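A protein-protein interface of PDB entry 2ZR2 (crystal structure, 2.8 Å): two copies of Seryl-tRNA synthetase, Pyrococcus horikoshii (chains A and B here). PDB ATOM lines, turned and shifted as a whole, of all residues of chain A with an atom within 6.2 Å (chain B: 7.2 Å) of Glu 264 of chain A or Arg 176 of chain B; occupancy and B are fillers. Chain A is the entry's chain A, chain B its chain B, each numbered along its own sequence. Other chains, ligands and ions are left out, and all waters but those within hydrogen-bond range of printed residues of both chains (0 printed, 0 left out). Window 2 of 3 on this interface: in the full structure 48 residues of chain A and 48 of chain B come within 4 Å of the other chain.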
ATOM      1  N   GLY A 259      13.666  21.355   9.028  1.00  0.00           N
ATOM      2  CA  GLY A 259      13.284  20.810  10.308  1.00  0.00           C
ATOM      3  C   GLY A 259      11.979  21.418  10.772  1.00  0.00           C
ATOM      4  O   GLY A 259      11.240  20.821  11.561  1.00  0.00           O
ATOM      5  N   MET A 260      11.691  22.609  10.269  1.00  0.00           N
ATOM      6  CA  MET A 260      10.477  23.318  10.638  1.00  0.00           C
ATOM      7  C   MET A 260       9.187  22.491  10.608  1.00  0.00           C
ATOM      8  O   MET A 260       8.278  22.752  11.380  1.00  0.00           O
ATOM      9  CB  MET A 260      10.326  24.549   9.751  1.00  0.00           C
ATOM     10  CG  MET A 260       9.057  25.336   9.974  1.00  0.00           C
ATOM     11  SD  MET A 260       8.954  26.713   8.809  1.00  0.00           S
ATOM     12  CE  MET A 260       8.480  28.013   9.919  1.00  0.00           C
ATOM     13  N   HIS A 261       9.099  21.498   9.729  1.00  0.00           N
ATOM     14  CA  HIS A 261       7.894  20.675   9.646  1.00  0.00           C
ATOM     15  C   HIS A 261       8.175  19.191   9.853  1.00  0.00           C
ATOM     16  O   HIS A 261       7.474  18.329   9.328  1.00  0.00           O
ATOM     17  CB  HIS A 261       7.197  20.887   8.301  1.00  0.00           C
ATOM     18  CG  HIS A 261       6.577  22.238   8.153  1.00  0.00           C
ATOM     19  ND1 HIS A 261       5.501  22.649   8.911  1.00  0.00           N
ATOM     20  CD2 HIS A 261       6.896  23.284   7.355  1.00  0.00           C
ATOM     21  CE1 HIS A 261       5.189  23.892   8.588  1.00  0.00           C
ATOM     22  NE2 HIS A 261       6.020  24.300   7.646  1.00  0.00           N
ATOM     23  N   ALA A 262       9.211  18.896  10.624  1.00  0.00           N
ATOM     24  CA  ALA A 262       9.562  17.515  10.909  1.00  0.00           C
ATOM     25  C   ALA A 262       8.395  16.904  11.685  1.00  0.00           C
ATOM     26  O   ALA A 262       7.802  17.564  12.540  1.00  0.00           O
ATOM     27  CB  ALA A 262      10.836  17.473  11.734  1.00  0.00           C
ATOM     28  N   ASN A 263       8.069  15.650  11.373  1.00  0.00           N
ATOM     29  CA  ASN A 263       6.974  14.908  12.011  1.00  0.00           C
ATOM     30  C   ASN A 263       5.616  15.566  11.828  1.00  0.00           C
ATOM     31  O   ASN A 263       4.914  15.819  12.784  1.00  0.00           O
ATOM     32  CB  ASN A 263       7.239  14.697  13.512  1.00  0.00           C
ATOM     33  CG  ASN A 263       8.376  13.715  13.779  1.00  0.00           C
ATOM     34  OD1 ASN A 263       8.381  12.600  13.262  1.00  0.00           O
ATOM     35  ND2 ASN A 263       9.341  14.126  14.599  1.00  0.00           N
ATOM     36  N   GLU A 264       5.252  15.859  10.593  1.00  0.00           N
ATOM     37  CA  GLU A 264       3.965  16.465  10.313  1.00  0.00           C
ATOM     38  C   GLU A 264       3.366  15.759   9.116  1.00  0.00           C
ATOM     39  O   GLU A 264       4.018  14.941   8.455  1.00  0.00           O
ATOM     40  CB  GLU A 264       4.096  17.952   9.962  1.00  0.00           C
ATOM     41  CG  GLU A 264       4.528  18.879  11.102  1.00  0.00           C
ATOM     42  CD  GLU A 264       4.344  20.359  10.755  1.00  0.00           C
ATOM     43  OE1 GLU A 264       4.859  21.218  11.504  1.00  0.00           O
ATOM     44  OE2 GLU A 264       3.676  20.662   9.737  1.00  0.00           O
ATOM     45  N   ILE A 265       2.101  16.061   8.866  1.00  0.00           N
ATOM     46  CA  ILE A 265       1.403  15.527   7.712  1.00  0.00           C
ATOM     47  C   ILE A 265       0.748  16.776   7.191  1.00  0.00           C
ATOM     48  O   ILE A 265      -0.201  17.280   7.787  1.00  0.00           O
ATOM     49  CB  ILE A 265       0.330  14.494   8.080  1.00  0.00           C
ATOM     50  CG1 ILE A 265       0.995  13.275   8.731  1.00  0.00           C
ATOM     51  CG2 ILE A 265      -0.441  14.087   6.818  1.00  0.00           C
ATOM     52  CD1 ILE A 265       0.047  12.185   9.119  1.00  0.00           C
ATOM     53  N   LEU A 266       1.288  17.304   6.104  1.00  0.00           N
ATOM     54  CA  LEU A 266       0.761  18.530   5.547  1.00  0.00           C
ATOM     55  C   LEU A 266      -0.547  18.298   4.803  1.00  0.00           C
ATOM     56  O   LEU A 266      -0.913  17.153   4.503  1.00  0.00           O
ATOM     57  CB  LEU A 266       1.800  19.148   4.608  1.00  0.00           C
ATOM     58  CG  LEU A 266       3.180  19.403   5.210  1.00  0.00           C
ATOM     59  CD1 LEU A 266       4.065  20.040   4.158  1.00  0.00           C
ATOM     60  CD2 LEU A 266       3.058  20.310   6.421  1.00  0.00           C
ATOM     61  N   LEU A 385      13.062  13.132   8.123  1.00  0.00           N
ATOM     62  CA  LEU A 385      12.354  13.997   9.063  1.00  0.00           C
ATOM     63  C   LEU A 385      10.889  13.643   9.249  1.00  0.00           C
ATOM     64  O   LEU A 385      10.206  14.261  10.061  1.00  0.00           O
ATOM     65  CB  LEU A 385      12.458  15.446   8.611  1.00  0.00           C
ATOM     66  CG  LEU A 385      13.888  15.962   8.587  1.00  0.00           C
ATOM     67  CD1 LEU A 385      13.913  17.397   8.079  1.00  0.00           C
ATOM     68  CD2 LEU A 385      14.459  15.855   9.994  1.00  0.00           C
ATOM     69  N   ASN A 386      10.419  12.647   8.498  1.00  0.00           N
ATOM     70  CA  ASN A 386       9.029  12.199   8.546  1.00  0.00           C
ATOM     71  C   ASN A 386       8.109  13.357   8.154  1.00  0.00           C
ATOM     72  O   ASN A 386       7.298  13.829   8.942  1.00  0.00           O
ATOM     73  CB  ASN A 386       8.705  11.666   9.948  1.00  0.00           C
ATOM     74  CG  ASN A 386       7.269  11.182  10.082  1.00  0.00           C
ATOM     75  OD1 ASN A 386       6.672  10.705   9.117  1.00  0.00           O
ATOM     76  ND2 ASN A 386       6.715  11.289  11.287  1.00  0.00           N
ATOM     77  N   ILE A 387       8.256  13.825   6.925  1.00  0.00           N
ATOM     78  CA  ILE A 387       7.450  14.931   6.456  1.00  0.00           C
ATOM     79  C   ILE A 387       6.564  14.419   5.335  1.00  0.00           C
ATOM     80  O   ILE A 387       6.986  14.293   4.184  1.00  0.00           O
ATOM     81  CB  ILE A 387       8.338  16.085   5.957  1.00  0.00           C
ATOM     82  CG1 ILE A 387       9.300  16.501   7.056  1.00  0.00           C
ATOM     83  CG2 ILE A 387       7.511  17.308   5.634  1.00  0.00           C
ATOM     84  CD1 ILE A 387      10.116  17.686   6.664  1.00  0.00           C
ATOM     85  N   ARG A 388       5.325  14.112   5.704  1.00  0.00           N
ATOM     86  CA  ARG A 388       4.343  13.591   4.773  1.00  0.00           C
ATOM     87  C   ARG A 388       3.215  14.570   4.550  1.00  0.00           C
ATOM     88  O   ARG A 388       3.117  15.604   5.219  1.00  0.00           O
ATOM     89  CB  ARG A 388       3.756  12.293   5.310  1.00  0.00           C
ATOM     90  CG  ARG A 388       4.740  11.167   5.400  1.00  0.00           C
ATOM     91  CD  ARG A 388       4.124  10.003   6.104  1.00  0.00           C
ATOM     92  NE  ARG A 388       3.855  10.324   7.497  1.00  0.00           N
ATOM     93  CZ  ARG A 388       3.277   9.484   8.349  1.00  0.00           C
ATOM     94  NH1 ARG A 388       3.070   9.851   9.609  1.00  0.00           N
ATOM     95  NH2 ARG A 388       2.898   8.282   7.935  1.00  0.00           N
ATOM     96  N   PHE A 389       2.357  14.224   3.602  1.00  0.00           N
ATOM     97  CA  PHE A 389       1.209  15.049   3.290  1.00  0.00           C
ATOM     98  C   PHE A 389       0.093  14.133   2.811  1.00  0.00           C
ATOM     99  O   PHE A 389       0.342  13.002   2.387  1.00  0.00           O
ATOM    100  CB  PHE A 389       1.552  16.058   2.193  1.00  0.00           C
ATOM    101  CG  PHE A 389       1.610  15.455   0.825  1.00  0.00           C
ATOM    102  CD1 PHE A 389       2.552  14.481   0.525  1.00  0.00           C
ATOM    103  CD2 PHE A 389       0.686  15.826  -0.146  1.00  0.00           C
ATOM    104  CE1 PHE A 389       2.576  13.880  -0.716  1.00  0.00           C
ATOM    105  CE2 PHE A 389       0.696  15.235  -1.394  1.00  0.00           C
ATOM    106  CZ  PHE A 389       1.645  14.256  -1.682  1.00  0.00           C
ATOM    107  N   ASP B 173       6.704  31.707  14.874  1.00  0.00           N
ATOM    108  CA  ASP B 173       6.252  30.347  15.167  1.00  0.00           C
ATOM    109  C   ASP B 173       7.147  29.878  16.307  1.00  0.00           C
ATOM    110  O   ASP B 173       8.351  29.709  16.117  1.00  0.00           O
ATOM    111  CB  ASP B 173       6.436  29.414  13.963  1.00  0.00           C
ATOM    112  CG  ASP B 173       5.930  27.976  14.235  1.00  0.00           C
ATOM    113  OD1 ASP B 173       6.262  27.388  15.301  1.00  0.00           O
ATOM    114  OD2 ASP B 173       5.205  27.427  13.365  1.00  0.00           O
ATOM    115  N   PHE B 174       6.573  29.677  17.492  1.00  0.00           N
ATOM    116  CA  PHE B 174       7.376  29.246  18.631  1.00  0.00           C
ATOM    117  C   PHE B 174       7.370  27.750  18.830  1.00  0.00           C
ATOM    118  O   PHE B 174       8.385  27.143  19.181  1.00  0.00           O
ATOM    119  CB  PHE B 174       6.908  29.944  19.907  1.00  0.00           C
ATOM    120  CG  PHE B 174       7.224  31.414  19.939  1.00  0.00           C
ATOM    121  CD1 PHE B 174       6.269  32.357  19.557  1.00  0.00           C
ATOM    122  CD2 PHE B 174       8.494  31.856  20.337  1.00  0.00           C
ATOM    123  CE1 PHE B 174       6.565  33.719  19.574  1.00  0.00           C
ATOM    124  CE2 PHE B 174       8.809  33.207  20.359  1.00  0.00           C
ATOM    125  CZ  PHE B 174       7.839  34.146  19.977  1.00  0.00           C
ATOM    126  N   ALA B 175       6.216  27.153  18.597  1.00  0.00           N
ATOM    127  CA  ALA B 175       6.067  25.715  18.750  1.00  0.00           C
ATOM    128  C   ALA B 175       7.090  24.934  17.919  1.00  0.00           C
ATOM    129  O   ALA B 175       7.766  24.036  18.426  1.00  0.00           O
ATOM    130  CB  ALA B 175       4.657  25.315  18.356  1.00  0.00           C
ATOM    131  N   ARG B 176       7.203  25.273  16.641  1.00  0.00           N
ATOM    132  CA  ARG B 176       8.140  24.561  15.789  1.00  0.00           C
ATOM    133  C   ARG B 176       9.602  24.807  16.171  1.00  0.00           C
ATOM    134  O   ARG B 176      10.435  23.901  16.081  1.00  0.00           O
ATOM    135  CB  ARG B 176       7.867  24.904  14.330  1.00  0.00           C
ATOM    136  CG  ARG B 176       6.510  24.409  13.884  1.00  0.00           C
ATOM    137  CD  ARG B 176       6.365  24.475  12.382  1.00  0.00           C
ATOM    138  NE  ARG B 176       5.237  23.677  11.917  1.00  0.00           N
ATOM    139  CZ  ARG B 176       3.987  24.123  11.839  1.00  0.00           C
ATOM    140  NH1 ARG B 176       3.027  23.315  11.409  1.00  0.00           N
ATOM    141  NH2 ARG B 176       3.696  25.380  12.172  1.00  0.00           N
ATOM    142  N   ALA B 177       9.914  26.021  16.612  1.00  0.00           N
ATOM    143  CA  ALA B 177      11.274  26.312  17.045  1.00  0.00           C
ATOM    144  C   ALA B 177      11.608  25.429  18.252  1.00  0.00           C
ATOM    145  O   ALA B 177      12.735  24.978  18.416  1.00  0.00           O
ATOM    146  CB  ALA B 177      11.405  27.785  17.415  1.00  0.00           C
ATOM    147  N   ALA B 178      10.626  25.186  19.107  1.00  0.00           N
ATOM    148  CA  ALA B 178      10.862  24.348  20.271  1.00  0.00           C
ATOM    149  C   ALA B 178      11.108  22.898  19.839  1.00  0.00           C
ATOM    150  O   ALA B 178      11.896  22.174  20.451  1.00  0.00           O
ATOM    151  CB  ALA B 178       9.688  24.421  21.195  1.00  0.00           C
ATOM    152  N   LYS B 179      10.432  22.482  18.778  1.00  0.00           N
ATOM    153  CA  LYS B 179      10.585  21.128  18.264  1.00  0.00           C
ATOM    154  C   LYS B 179      12.007  20.974  17.733  1.00  0.00           C
ATOM    155  O   LYS B 179      12.755  20.064  18.069  1.00  0.00           O
ATOM    156  CB  LYS B 179       9.582  20.919  17.115  1.00  0.00           C
ATOM    157  CG  LYS B 179       9.665  19.563  16.417  1.00  0.00           C
ATOM    158  CD  LYS B 179       9.360  19.659  14.920  1.00  0.00           C
ATOM    159  CE  LYS B 179       7.978  20.195  14.604  1.00  0.00           C
ATOM    160  NZ  LYS B 179       7.810  20.369  13.131  1.00  0.00           N
ATOM    161  N   VAL B 180      12.349  21.935  16.900  1.00  0.00           N
ATOM    162  CA  VAL B 180      13.600  22.019  16.197  1.00  0.00           C
ATOM    163  C   VAL B 180      14.871  22.331  16.987  1.00  0.00           C
ATOM    164  O   VAL B 180      15.933  21.780  16.687  1.00  0.00           O
ATOM    165  CB  VAL B 180      13.400  23.050  15.081  1.00  0.00           C
ATOM    166  CG1 VAL B 180      14.576  23.947  14.978  1.00  0.00           C
ATOM    167  CG2 VAL B 180      13.093  22.341  13.789  1.00  0.00           C
ATOM    168  N   SER B 181      14.773  23.206  17.987  1.00  0.00           N
ATOM    169  CA  SER B 181      15.949  23.622  18.758  1.00  0.00           C
ATOM    170  C   SER B 181      15.782  23.569  20.270  1.00  0.00           C
ATOM    171  O   SER B 181      16.748  23.417  21.011  1.00  0.00           O
ATOM    172  CB  SER B 181      16.344  25.067  18.378  1.00  0.00           C
ATOM    173  OG  SER B 181      16.506  25.226  16.981  1.00  0.00           O
ATOM    174  N   GLY B 182      14.557  23.716  20.734  1.00  0.00           N
ATOM    175  CA  GLY B 182      14.327  23.723  22.158  1.00  0.00           C
ATOM    176  C   GLY B 182      13.613  25.022  22.476  1.00  0.00           C
ATOM    177  O   GLY B 182      13.215  25.778  21.568  1.00  0.00           O
ATOM    178  N   PHE B 185      13.846  29.737  21.600  1.00  0.00           N
ATOM    179  CA  PHE B 185      14.301  29.834  20.211  1.00  0.00           C
ATOM    180  C   PHE B 185      13.023  30.209  19.465  1.00  0.00           C
ATOM    181  O   PHE B 185      11.931  30.110  20.012  1.00  0.00           O
ATOM    182  CB  PHE B 185      14.869  28.506  19.679  1.00  0.00           C
ATOM    183  CG  PHE B 185      16.329  28.312  19.995  1.00  0.00           C
ATOM    184  CD1 PHE B 185      16.734  27.414  20.982  1.00  0.00           C
ATOM    185  CD2 PHE B 185      17.299  29.100  19.359  1.00  0.00           C
ATOM    186  CE1 PHE B 185      18.079  27.306  21.338  1.00  0.00           C
ATOM    187  CE2 PHE B 185      18.638  29.003  19.703  1.00  0.00           C
ATOM    188  CZ  PHE B 185      19.036  28.100  20.702  1.00  0.00           C
ATOM    189  N   TYR B 186      13.128  30.631  18.223  1.00  0.00           N
ATOM    190  CA  TYR B 186      11.922  31.038  17.535  1.00  0.00           C
ATOM    191  C   TYR B 186      12.165  31.161  16.058  1.00  0.00           C
ATOM    192  O   TYR B 186      13.306  31.162  15.603  1.00  0.00           O
ATOM    193  CB  TYR B 186      11.507  32.411  18.032  1.00  0.00           C
ATOM    194  CG  TYR B 186      12.632  33.412  17.880  1.00  0.00           C
ATOM    195  CD1 TYR B 186      13.497  33.675  18.938  1.00  0.00           C
ATOM    196  CD2 TYR B 186      12.913  34.005  16.641  1.00  0.00           C
ATOM    197  CE1 TYR B 186      14.620  34.492  18.770  1.00  0.00           C
ATOM    198  CE2 TYR B 186      14.033  34.816  16.461  1.00  0.00           C
ATOM    199  CZ  TYR B 186      14.886  35.050  17.532  1.00  0.00           C
ATOM    200  OH  TYR B 186      16.038  35.786  17.376  1.00  0.00           O
ATOM    201  N   TYR B 187      11.073  31.281  15.318  1.00  0.00           N
ATOM    202  CA  TYR B 187      11.130  31.511  13.890  1.00  0.00           C
ATOM    203  C   TYR B 187      10.403  32.824  13.756  1.00  0.00           C
ATOM    204  O   TYR B 187       9.287  32.944  14.242  1.00  0.00           O
ATOM    205  CB  TYR B 187      10.347  30.476  13.068  1.00  0.00           C
ATOM    206  CG  TYR B 187      10.988  29.113  12.895  1.00  0.00           C
ATOM    207  CD1 TYR B 187      10.960  28.190  13.921  1.00  0.00           C
ATOM    208  CD2 TYR B 187      11.570  28.729  11.677  1.00  0.00           C
ATOM    209  CE1 TYR B 187      11.479  26.919  13.761  1.00  0.00           C
ATOM    210  CE2 TYR B 187      12.104  27.445  11.506  1.00  0.00           C
ATOM    211  CZ  TYR B 187      12.053  26.545  12.564  1.00  0.00           C
ATOM    212  OH  TYR B 187      12.587  25.269  12.482  1.00  0.00           O
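NZ of Lys 179 of chain B is in hydrogen-bond range of O of Met 260 of chain A (3.0 Å).
The side-chain amino group of Lys 179 of chain B lies within salt-bridge range of the side-chain carboxylate of Glu 264 of chain A (3.5 Å).
The side-chain amino group (NZ) of Lys 179 of chain B lies within hydrogen-bond range of the backbone carbonyl oxygen (O) of Ala 262 of chain A (2.9 Å).
ND1 of His 261 of chain A is in hydrogen-bond range of NE of Arg 176 of chain B, at 3.2 Å.
NE of Arg 176 of chain B is in salt-bridge range of OE1 of Glu 264 of chain A, 2.5 Å away.
The backbone carbonyl oxygen of Met 260 of chain A lies close to the guanidinium group of Arg 176 of chain B (3.2 Å).
No position is printed for both chains.
Of the 11 pairs that touch across the chains among the printed residues, none has its exchanged pair printed and touching as well.
Printed residues of chain B that touch a printed residue of chain A: Arg 176, Lys 179, Val 180 and Tyr 187.
Hydrophobic or aromatic side chains of chain B that line the printed part of chain A: Val 180 and Tyr 187.
Hydrophobic or aromatic side chains of chain A within 4 Å of the printed part of chain B: Met 260 and His 261.
Among the printed residues, merely in contact across the chains: Gly 259 of chain A with Lys 179 of chain B (3.8 Å), Gly 259 of chain A with Val 180 of chain B (3.3 Å), Met 260 of chain A with Val 180 of chain B (3.8 Å), Met 260 of chain A with Tyr 187 of chain B (3.4 Å) and His 261 of chain A with Lys 179 of chain B (3.5 Å).
Of the printed residues of chain B, Gly 259 of chain A touches Lys 179 and Val 180.
Of the printed residues of chain B, Ala 262 of chain A touches Lys 179.
Of the printed residues of chain B, Glu 264 of chain A touches Arg 176 (2.5 Å) and Lys 179 (3.5 Å).
Arg 176 of chain B touches just these residues of chain A: Met 260, His 261 and Glu 264.
Of the printed residues of chain A, Lys 179 of chain B touches Gly 259 (3.8 Å), Met 260 (3.0 Å), His 261 (3.5 Å), Ala 262 (2.9 Å) and Glu 264 (3.5 Å).
The nearest residue of chain B that does not touch Glu 264 of chain A is Asp 173 of chain B (6.5 Å).
The nearest residue of chain A that does not touch Arg 176 of chain B is Gly 259 of chain A (5.5 Å).
The nearest printed residue of chain B that does not touch Ala 262 of chain A is Val 180 of chain B (5.7 Å).
OD2 of Asp 173 of chain B lies within salt-bridge range of NH2 of Arg 176 of chain B (2.8 Å).
The backbone NH of Glu 264 of chain A lies within hydrogen-bond range of the backbone carbonyl oxygen of Asn 386 of chain A (3.3 Å).
The backbone NH of Arg 388 of chain A is in hydrogen-bond range of the backbone carbonyl oxygen of Glu 264 of chain A (3.2 Å).
ND1 of His 261 of chain A is in hydrogen-bond range of OE2 of Glu 264 of chain A, 2.8 Å away.
N of Asp 173 of chain B sits at hydrogen-bond distance from O of Tyr 187 of chain B (2.9 Å).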
